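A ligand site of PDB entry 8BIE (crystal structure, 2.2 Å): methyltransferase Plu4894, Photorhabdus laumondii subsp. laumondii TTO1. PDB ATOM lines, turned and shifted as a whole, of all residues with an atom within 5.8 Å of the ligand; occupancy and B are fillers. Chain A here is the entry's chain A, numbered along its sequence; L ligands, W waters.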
ATOM      1  N   PHE A 127       0.365  -0.362 -14.643  1.00  0.00           N
ATOM      2  CA  PHE A 127       0.462  -0.879 -16.041  1.00  0.00           C
ATOM      3  C   PHE A 127      -0.096  -2.313 -16.114  1.00  0.00           C
ATOM      4  O   PHE A 127      -0.739  -2.638 -17.127  1.00  0.00           O
ATOM      5  CB  PHE A 127       1.890  -0.775 -16.562  1.00  0.00           C
ATOM      6  CG  PHE A 127       2.375   0.640 -16.771  1.00  0.00           C
ATOM      7  CD1 PHE A 127       1.636   1.533 -17.540  1.00  0.00           C
ATOM      8  CD2 PHE A 127       3.557   1.086 -16.205  1.00  0.00           C
ATOM      9  CE1 PHE A 127       2.075   2.842 -17.730  1.00  0.00           C
ATOM     10  CE2 PHE A 127       3.991   2.387 -16.390  1.00  0.00           C
ATOM     11  CZ  PHE A 127       3.254   3.257 -17.150  1.00  0.00           C
ATOM     12  N   PHE A 140      -6.311   6.686 -20.441  1.00  0.00           N
ATOM     13  CA  PHE A 140      -4.870   6.921 -20.154  1.00  0.00           C
ATOM     14  C   PHE A 140      -4.103   7.067 -21.466  1.00  0.00           C
ATOM     15  O   PHE A 140      -3.397   8.086 -21.639  1.00  0.00           O
ATOM     16  CB  PHE A 140      -4.280   5.805 -19.293  1.00  0.00           C
ATOM     17  CG  PHE A 140      -2.800   5.959 -19.006  1.00  0.00           C
ATOM     18  CD1 PHE A 140      -2.359   6.772 -17.970  1.00  0.00           C
ATOM     19  CD2 PHE A 140      -1.857   5.309 -19.778  1.00  0.00           C
ATOM     20  CE1 PHE A 140      -1.004   6.916 -17.723  1.00  0.00           C
ATOM     21  CE2 PHE A 140      -0.502   5.454 -19.531  1.00  0.00           C
ATOM     22  CZ  PHE A 140      -0.073   6.260 -18.497  1.00  0.00           C
ATOM     23  N   ASP A 141      -4.249   6.085 -22.370  1.00  0.00           N
ATOM     24  CA  ASP A 141      -3.561   6.008 -23.691  1.00  0.00           C
ATOM     25  C   ASP A 141      -3.866   7.273 -24.507  1.00  0.00           C
ATOM     26  O   ASP A 141      -2.911   7.851 -25.056  1.00  0.00           O
ATOM     27  CB  ASP A 141      -3.984   4.764 -24.466  1.00  0.00           C
ATOM     28  CG  ASP A 141      -3.307   3.472 -24.033  1.00  0.00           C
ATOM     29  OD1 ASP A 141      -2.288   3.559 -23.305  1.00  0.00           O
ATOM     30  OD2 ASP A 141      -3.781   2.392 -24.426  1.00  0.00           O
ATOM     31  N   MET A 144      -2.128  10.399 -23.131  1.00  0.00           N
ATOM     32  CA  MET A 144      -0.676  10.307 -23.463  1.00  0.00           C
ATOM     33  C   MET A 144      -0.440  10.842 -24.893  1.00  0.00           C
ATOM     34  O   MET A 144       0.573  11.532 -25.093  1.00  0.00           O
ATOM     35  CB  MET A 144      -0.166   8.868 -23.380  1.00  0.00           C
ATOM     36  CG  MET A 144       0.014   8.345 -21.963  1.00  0.00           C
ATOM     37  SD  MET A 144       1.062   9.406 -20.923  1.00  0.00           S
ATOM     38  CE  MET A 144      -0.190  10.292 -19.995  1.00  0.00           C
ATOM     39  N   SER A 145      -1.338  10.516 -25.832  1.00  0.00           N
ATOM     40  CA  SER A 145      -1.270  10.938 -27.252  1.00  0.00           C
ATOM     41  C   SER A 145      -1.457  12.454 -27.367  1.00  0.00           C
ATOM     42  O   SER A 145      -0.686  13.088 -28.110  1.00  0.00           O
ATOM     43  CB  SER A 145      -2.293  10.208 -28.084  1.00  0.00           C
ATOM     44  OG  SER A 145      -2.171   8.811 -27.915  1.00  0.00           O
ATOM     45  N   SER A 148       1.691  14.076 -26.482  1.00  0.00           N
ATOM     46  CA  SER A 148       2.645  14.004 -27.618  1.00  0.00           C
ATOM     47  C   SER A 148       2.297  15.051 -28.678  1.00  0.00           C
ATOM     48  O   SER A 148       3.242  15.665 -29.224  1.00  0.00           O
ATOM     49  CB  SER A 148       2.688  12.617 -28.211  1.00  0.00           C
ATOM     50  OG  SER A 148       3.290  11.695 -27.310  1.00  0.00           O
ATOM     51  N   ASP A 169      11.063   3.920 -30.382  1.00  0.00           N
ATOM     52  CA  ASP A 169      10.388   4.550 -29.225  1.00  0.00           C
ATOM     53  C   ASP A 169      10.171   3.486 -28.145  1.00  0.00           C
ATOM     54  O   ASP A 169       9.231   2.675 -28.280  1.00  0.00           O
ATOM     55  CB  ASP A 169       9.067   5.209 -29.645  1.00  0.00           C
ATOM     56  CG  ASP A 169       8.483   6.179 -28.628  1.00  0.00           C
ATOM     57  OD1 ASP A 169       9.213   6.534 -27.670  1.00  0.00           O
ATOM     58  OD2 ASP A 169       7.320   6.577 -28.799  1.00  0.00           O
ATOM     59  N   ILE A 170      11.032   3.475 -27.114  1.00  0.00           N
ATOM     60  CA  ILE A 170      10.978   2.500 -25.977  1.00  0.00           C
ATOM     61  C   ILE A 170       9.869   2.939 -25.025  1.00  0.00           C
ATOM     62  O   ILE A 170       9.953   4.071 -24.510  1.00  0.00           O
ATOM     63  CB  ILE A 170      12.347   2.399 -25.285  1.00  0.00           C
ATOM     64  CG1 ILE A 170      13.447   1.947 -26.244  1.00  0.00           C
ATOM     65  CG2 ILE A 170      12.280   1.480 -24.072  1.00  0.00           C
ATOM     66  CD1 ILE A 170      14.843   2.331 -25.809  1.00  0.00           C
ATOM     67  N   GLY A 171       8.868   2.075 -24.810  1.00  0.00           N
ATOM     68  CA  GLY A 171       7.644   2.394 -24.044  1.00  0.00           C
ATOM     69  C   GLY A 171       6.822   3.469 -24.741  1.00  0.00           C
ATOM     70  O   GLY A 171       6.333   4.378 -24.044  1.00  0.00           O
ATOM     71  N   GLY A 172       6.663   3.358 -26.065  1.00  0.00           N
ATOM     72  CA  GLY A 172       5.986   4.358 -26.922  1.00  0.00           C
ATOM     73  C   GLY A 172       4.478   4.188 -26.940  1.00  0.00           C
ATOM     74  O   GLY A 172       3.801   5.098 -27.463  1.00  0.00           O
ATOM     75  N   GLY A 173       3.963   3.072 -26.413  1.00  0.00           N
ATOM     76  CA  GLY A 173       2.519   2.817 -26.237  1.00  0.00           C
ATOM     77  C   GLY A 173       1.772   2.757 -27.565  1.00  0.00           C
ATOM     78  O   GLY A 173       2.023   1.822 -28.341  1.00  0.00           O
ATOM     79  N   LEU A 193       8.435  -0.109 -29.120  1.00  0.00           N
ATOM     80  CA  LEU A 193       8.526  -1.249 -28.160  1.00  0.00           C
ATOM     81  C   LEU A 193       7.677  -0.931 -26.929  1.00  0.00           C
ATOM     82  O   LEU A 193       7.833   0.170 -26.366  1.00  0.00           O
ATOM     83  CB  LEU A 193       9.990  -1.476 -27.784  1.00  0.00           C
ATOM     84  CG  LEU A 193      10.255  -2.635 -26.819  1.00  0.00           C
ATOM     85  CD1 LEU A 193      11.607  -3.282 -27.106  1.00  0.00           C
ATOM     86  CD2 LEU A 193      10.188  -2.175 -25.373  1.00  0.00           C
ATOM     87  N   ASP A 194       6.810  -1.861 -26.525  1.00  0.00           N
ATOM     88  CA  ASP A 194       5.926  -1.735 -25.336  1.00  0.00           C
ATOM     89  C   ASP A 194       5.360  -3.119 -24.990  1.00  0.00           C
ATOM     90  O   ASP A 194       5.793  -4.112 -25.619  1.00  0.00           O
ATOM     91  CB  ASP A 194       4.815  -0.711 -25.576  1.00  0.00           C
ATOM     92  CG  ASP A 194       4.366   0.016 -24.326  1.00  0.00           C
ATOM     93  OD1 ASP A 194       3.899  -0.660 -23.390  1.00  0.00           O
ATOM     94  OD2 ASP A 194       4.482   1.260 -24.291  1.00  0.00           O
ATOM     95  N   ARG A 195       4.448  -3.187 -24.012  1.00  0.00           N
ATOM     96  CA  ARG A 195       3.720  -4.420 -23.597  1.00  0.00           C
ATOM     97  C   ARG A 195       2.367  -4.446 -24.302  1.00  0.00           C
ATOM     98  O   ARG A 195       1.480  -3.661 -23.906  1.00  0.00           O
ATOM     99  CB  ARG A 195       3.560  -4.457 -22.069  1.00  0.00           C
ATOM    100  CG  ARG A 195       4.865  -4.349 -21.305  1.00  0.00           C
ATOM    101  CD  ARG A 195       5.550  -5.693 -21.098  1.00  0.00           C
ATOM    102  NE  ARG A 195       4.948  -6.444 -19.994  1.00  0.00           N
ATOM    103  CZ  ARG A 195       5.554  -6.760 -18.854  1.00  0.00           C
ATOM    104  NH1 ARG A 195       4.891  -7.450 -17.935  1.00  0.00           N
ATOM    105  NH2 ARG A 195       6.806  -6.401 -18.613  1.00  0.00           N
ATOM    106  N   GLY A 210       7.875  -6.482 -26.304  1.00  0.00           N
ATOM    107  CA  GLY A 210       9.113  -6.743 -25.530  1.00  0.00           C
ATOM    108  C   GLY A 210       9.011  -6.221 -24.108  1.00  0.00           C
ATOM    109  O   GLY A 210       7.938  -5.716 -23.729  1.00  0.00           O
ATOM    110  N   ASP A 211      10.099  -6.364 -23.348  1.00  0.00           N
ATOM    111  CA  ASP A 211      10.258  -5.884 -21.953  1.00  0.00           C
ATOM    112  C   ASP A 211      11.584  -5.133 -21.871  1.00  0.00           C
ATOM    113  O   ASP A 211      12.640  -5.805 -21.973  1.00  0.00           O
ATOM    114  CB  ASP A 211      10.185  -7.066 -20.975  1.00  0.00           C
ATOM    115  CG  ASP A 211      10.260  -6.675 -19.508  1.00  0.00           C
ATOM    116  OD1 ASP A 211      10.193  -7.593 -18.663  1.00  0.00           O
ATOM    117  OD2 ASP A 211      10.372  -5.475 -19.222  1.00  0.00           O
ATOM    118  N   PHE A 212      11.558  -3.809 -21.709  1.00  0.00           N
ATOM    119  CA  PHE A 212      12.777  -2.950 -21.699  1.00  0.00           C
ATOM    120  C   PHE A 212      13.584  -3.182 -20.406  1.00  0.00           C
ATOM    121  O   PHE A 212      14.706  -2.660 -20.325  1.00  0.00           O
ATOM    122  CB  PHE A 212      12.470  -1.473 -21.961  1.00  0.00           C
ATOM    123  CG  PHE A 212      11.437  -0.794 -21.087  1.00  0.00           C
ATOM    124  CD1 PHE A 212      11.544  -0.787 -19.703  1.00  0.00           C
ATOM    125  CD2 PHE A 212      10.393  -0.077 -21.660  1.00  0.00           C
ATOM    126  CE1 PHE A 212      10.613  -0.133 -18.911  1.00  0.00           C
ATOM    127  CE2 PHE A 212       9.466   0.585 -20.874  1.00  0.00           C
ATOM    128  CZ  PHE A 212       9.576   0.556 -19.499  1.00  0.00           C
ATOM    129  N   LEU A 213      13.032  -3.934 -19.444  1.00  0.00           N
ATOM    130  CA  LEU A 213      13.776  -4.388 -18.228  1.00  0.00           C
ATOM    131  C   LEU A 213      14.633  -5.613 -18.560  1.00  0.00           C
ATOM    132  O   LEU A 213      15.589  -5.876 -17.807  1.00  0.00           O
ATOM    133  CB  LEU A 213      12.789  -4.697 -17.108  1.00  0.00           C
ATOM    134  CG  LEU A 213      12.029  -3.493 -16.532  1.00  0.00           C
ATOM    135  CD1 LEU A 213      10.928  -3.959 -15.591  1.00  0.00           C
ATOM    136  CD2 LEU A 213      12.965  -2.536 -15.821  1.00  0.00           C
ATOM    137  N   LYS A 226      10.465   8.545 -23.760  1.00  0.00           N
ATOM    138  CA  LYS A 226       9.564   9.692 -23.469  1.00  0.00           C
ATOM    139  C   LYS A 226       8.635   9.317 -22.306  1.00  0.00           C
ATOM    140  O   LYS A 226       7.809   8.398 -22.492  1.00  0.00           O
ATOM    141  CB  LYS A 226       8.757  10.102 -24.695  1.00  0.00           C
ATOM    142  CG  LYS A 226       7.873  11.324 -24.505  1.00  0.00           C
ATOM    143  CD  LYS A 226       6.850  11.539 -25.601  1.00  0.00           C
ATOM    144  CE  LYS A 226       5.877  12.652 -25.291  1.00  0.00           C
ATOM    145  NZ  LYS A 226       4.894  12.260 -24.256  1.00  0.00           N
ATOM    146  N   ASP A 227       8.758  10.009 -21.174  1.00  0.00           N
ATOM    147  CA  ASP A 227       7.910   9.844 -19.958  1.00  0.00           C
ATOM    148  C   ASP A 227       7.958   8.387 -19.486  1.00  0.00           C
ATOM    149  O   ASP A 227       6.912   7.864 -19.054  1.00  0.00           O
ATOM    150  CB  ASP A 227       6.470  10.299 -20.224  1.00  0.00           C
ATOM    151  CG  ASP A 227       6.335  11.753 -20.621  1.00  0.00           C
ATOM    152  OD1 ASP A 227       7.190  12.563 -20.190  1.00  0.00           O
ATOM    153  OD2 ASP A 227       5.386  12.077 -21.355  1.00  0.00           O
ATOM    154  N   VAL A 228       9.141   7.753 -19.563  1.00  0.00           N
ATOM    155  CA  VAL A 228       9.389   6.353 -19.133  1.00  0.00           C
ATOM    156  C   VAL A 228      10.198   6.341 -17.832  1.00  0.00           C
ATOM    157  O   VAL A 228       9.725   5.733 -16.860  1.00  0.00           O
ATOM    158  CB  VAL A 228      10.077   5.538 -20.247  1.00  0.00           C
ATOM    159  CG1 VAL A 228      10.715   4.252 -19.717  1.00  0.00           C
ATOM    160  CG2 VAL A 228       9.118   5.211 -21.383  1.00  0.00           C
ATOM    161  N   ASP A 231       8.886   6.815 -14.264  1.00  0.00           N
ATOM    162  CA  ASP A 231       7.994   5.732 -13.762  1.00  0.00           C
ATOM    163  C   ASP A 231       8.737   4.795 -12.800  1.00  0.00           C
ATOM    164  O   ASP A 231       8.063   3.999 -12.126  1.00  0.00           O
ATOM    165  CB  ASP A 231       7.433   4.868 -14.901  1.00  0.00           C
ATOM    166  CG  ASP A 231       6.489   5.595 -15.850  1.00  0.00           C
ATOM    167  OD1 ASP A 231       5.891   6.609 -15.429  1.00  0.00           O
ATOM    168  OD2 ASP A 231       6.346   5.127 -16.993  1.00  0.00           O
ATOM    169  N   TRP A 232      10.076   4.877 -12.735  1.00  0.00           N
ATOM    170  CA  TRP A 232      10.940   3.815 -12.168  1.00  0.00           C
ATOM    171  C   TRP A 232      11.830   4.332 -11.039  1.00  0.00           C
ATOM    172  O   TRP A 232      12.193   5.525 -11.061  1.00  0.00           O
ATOM    173  CB  TRP A 232      11.783   3.168 -13.280  1.00  0.00           C
ATOM    174  CG  TRP A 232      10.935   2.511 -14.329  1.00  0.00           C
ATOM    175  CD1 TRP A 232      10.606   3.012 -15.549  1.00  0.00           C
ATOM    176  CD2 TRP A 232      10.275   1.240 -14.228  1.00  0.00           C
ATOM    177  NE1 TRP A 232       9.800   2.136 -16.230  1.00  0.00           N
ATOM    178  CE2 TRP A 232       9.581   1.042 -15.439  1.00  0.00           C
ATOM    179  CE3 TRP A 232      10.209   0.249 -13.239  1.00  0.00           C
ATOM    180  CZ2 TRP A 232       8.828  -0.111 -15.681  1.00  0.00           C
ATOM    181  CZ3 TRP A 232       9.471  -0.884 -13.477  1.00  0.00           C
ATOM    182  CH2 TRP A 232       8.790  -1.062 -14.686  1.00  0.00           C
HETATM  183  N1  LIG L   1       6.085   6.975 -24.097  1.00  0.00           N
HETATM  184  C1  LIG L   1       4.587   7.036 -24.081  1.00  0.00           C
HETATM  185  C2  LIG L   1       3.991   6.307 -22.869  1.00  0.00           C
HETATM  186  C3  LIG L   1       4.600   6.695 -21.531  1.00  0.00           C
HETATM  187  S1  LIG L   1       3.940   5.742 -20.141  1.00  0.00           S
HETATM  188  C4  LIG L   1       4.142   8.509 -24.062  1.00  0.00           C
HETATM  189  O1  LIG L   1       3.076   8.848 -24.570  1.00  0.00           O
HETATM  190  O2  LIG L   1       4.830   9.373 -23.526  1.00  0.00           O
HETATM  191  C5  LIG L   1       5.165   4.418 -19.955  1.00  0.00           C
HETATM  192  C6  LIG L   1       5.040   3.290 -20.962  1.00  0.00           C
HETATM  193  O3  LIG L   1       5.987   2.250 -20.620  1.00  0.00           O
HETATM  194  C7  LIG L   1       3.662   2.625 -21.026  1.00  0.00           C
HETATM  195  O4  LIG L   1       3.183   2.622 -22.369  1.00  0.00           O
HETATM  196  C8  LIG L   1       3.910   1.200 -20.507  1.00  0.00           C
HETATM  197  O5  LIG L   1       3.096   0.248 -21.144  1.00  0.00           O
HETATM  198  C9  LIG L   1       5.371   0.996 -20.857  1.00  0.00           C
HETATM  199  N2  LIG L   1       6.046  -0.019 -20.048  1.00  0.00           N
HETATM  200  C10 LIG L   1       6.008  -0.130 -18.682  1.00  0.00           C
HETATM  201  N3  LIG L   1       6.694  -1.140 -18.222  1.00  0.00           N
HETATM  202  C11 LIG L   1       7.240  -1.723 -19.355  1.00  0.00           C
HETATM  203  C12 LIG L   1       8.081  -2.844 -19.536  1.00  0.00           C
HETATM  204  N4  LIG L   1       8.549  -3.584 -18.531  1.00  0.00           N
HETATM  205  N5  LIG L   1       8.449  -3.158 -20.798  1.00  0.00           N
HETATM  206  C13 LIG L   1       7.982  -2.403 -21.801  1.00  0.00           C
HETATM  207  N6  LIG L   1       7.179  -1.340 -21.757  1.00  0.00           N
HETATM  208  C14 LIG L   1       6.843  -1.042 -20.490  1.00  0.00           C
HETATM  209  O   HOH W   1       7.402   2.940 -18.219  1.00  0.00           O
HETATM  210  O   HOH W   2       4.237   7.713 -17.444  1.00  0.00           O
HETATM  211  O   HOH W   3       6.415   8.034 -26.800  1.00  0.00           O
HETATM  212  O   HOH W   4       9.124   6.574 -25.096  1.00  0.00           O
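An oxygen (O5) of the ligand is in hydrogen-bond range of the side-chain carboxylate (OD1) of Asp 194. A nitrogen (N1) of the ligand lies within hydrogen-bond range of the backbone carbonyl oxygen of Gly 171. A nitrogen (N4) of the ligand sits at hydrogen-bond distance from the side-chain carboxylate of Asp 211 (2.7 Å). O of Lys 226 lies within hydrogen-bond range of N1 of the ligand (2.8 Å). O2 of the ligand lies within salt-bridge range of NZ of Lys 226, 3.0 Å away. N of Phe 212 is in hydrogen-bond range of N5 of the ligand, 3.3 Å away.
The backbone NH (N) of Gly 210 lies within hydrogen-bond range of the backbone carbonyl oxygen (O) of Asp 194, at 3.2 Å. The side-chain carboxylate of Asp 194 is in hydrogen-bond range of the backbone NH of Gly 173. The backbone NH (N) of Gly 171 sits at hydrogen-bond distance from the backbone carbonyl oxygen (O) of Leu 193. OD1 of Asp 211 lies within salt-bridge range of NH2 of Arg 195. The side-chain carboxylate (OD2) of Asp 211 lies close to the backbone NH (N) of Leu 213, at 3.1 Å. OD2 of Asp 227 is in salt-bridge range of NZ of Lys 226 (2.9 Å). The side-chain amino group (NZ) of Lys 226 lies close to the side-chain hydroxyl (OG) of Ser 148 (3.5 Å). The backbone NH of Gly 172 sits at hydrogen-bond distance from the backbone carbonyl oxygen of Leu 193.
NH2 of Arg 195 lies close to N4 of the ligand, 3.3 Å away. Residues that only touch the ligand: Asp 231 (3.3 Å), Met 144 (3.5 Å), Trp 232 (3.5 Å), Asp 227 (3.5 Å), Phe 127 (3.6 Å), Leu 213 (3.8 Å), Gly 210 (3.8 Å), Gly 172 (3.9 Å), Gly 173 (3.9 Å) and Ser 148 (3.96 Å). Hydrophobic or aromatic side chains that line the ligand: Phe 127, Met 144, Phe 212, Leu 213 and Trp 232. 16 residues have an atom within 4 Å of the ligand: Phe 127, Met 144, Ser 148, Gly 171, Gly 172, Gly 173, Asp 194, Arg 195, Gly 210, Asp 211, Phe 212, Leu 213, Lys 226, Asp 227, Asp 231 and Trp 232. The nearest printed residue that does not touch the ligand is Leu 193 (4.2 Å).
Water W1 lies within hydrogen-bond range of the side-chain carboxylate of Asp 231, an oxygen (O3) of the ligand and the indole nitrogen of Trp 232. Water W3 lies within hydrogen-bond range of the side-chain carboxylate (OD2) of Asp 169 and a nitrogen (N1) of the ligand. Water W4 lies within hydrogen-bond range of OD1 of Asp 169, O of Ile 170, N of Lys 226 and N1 of the ligand.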
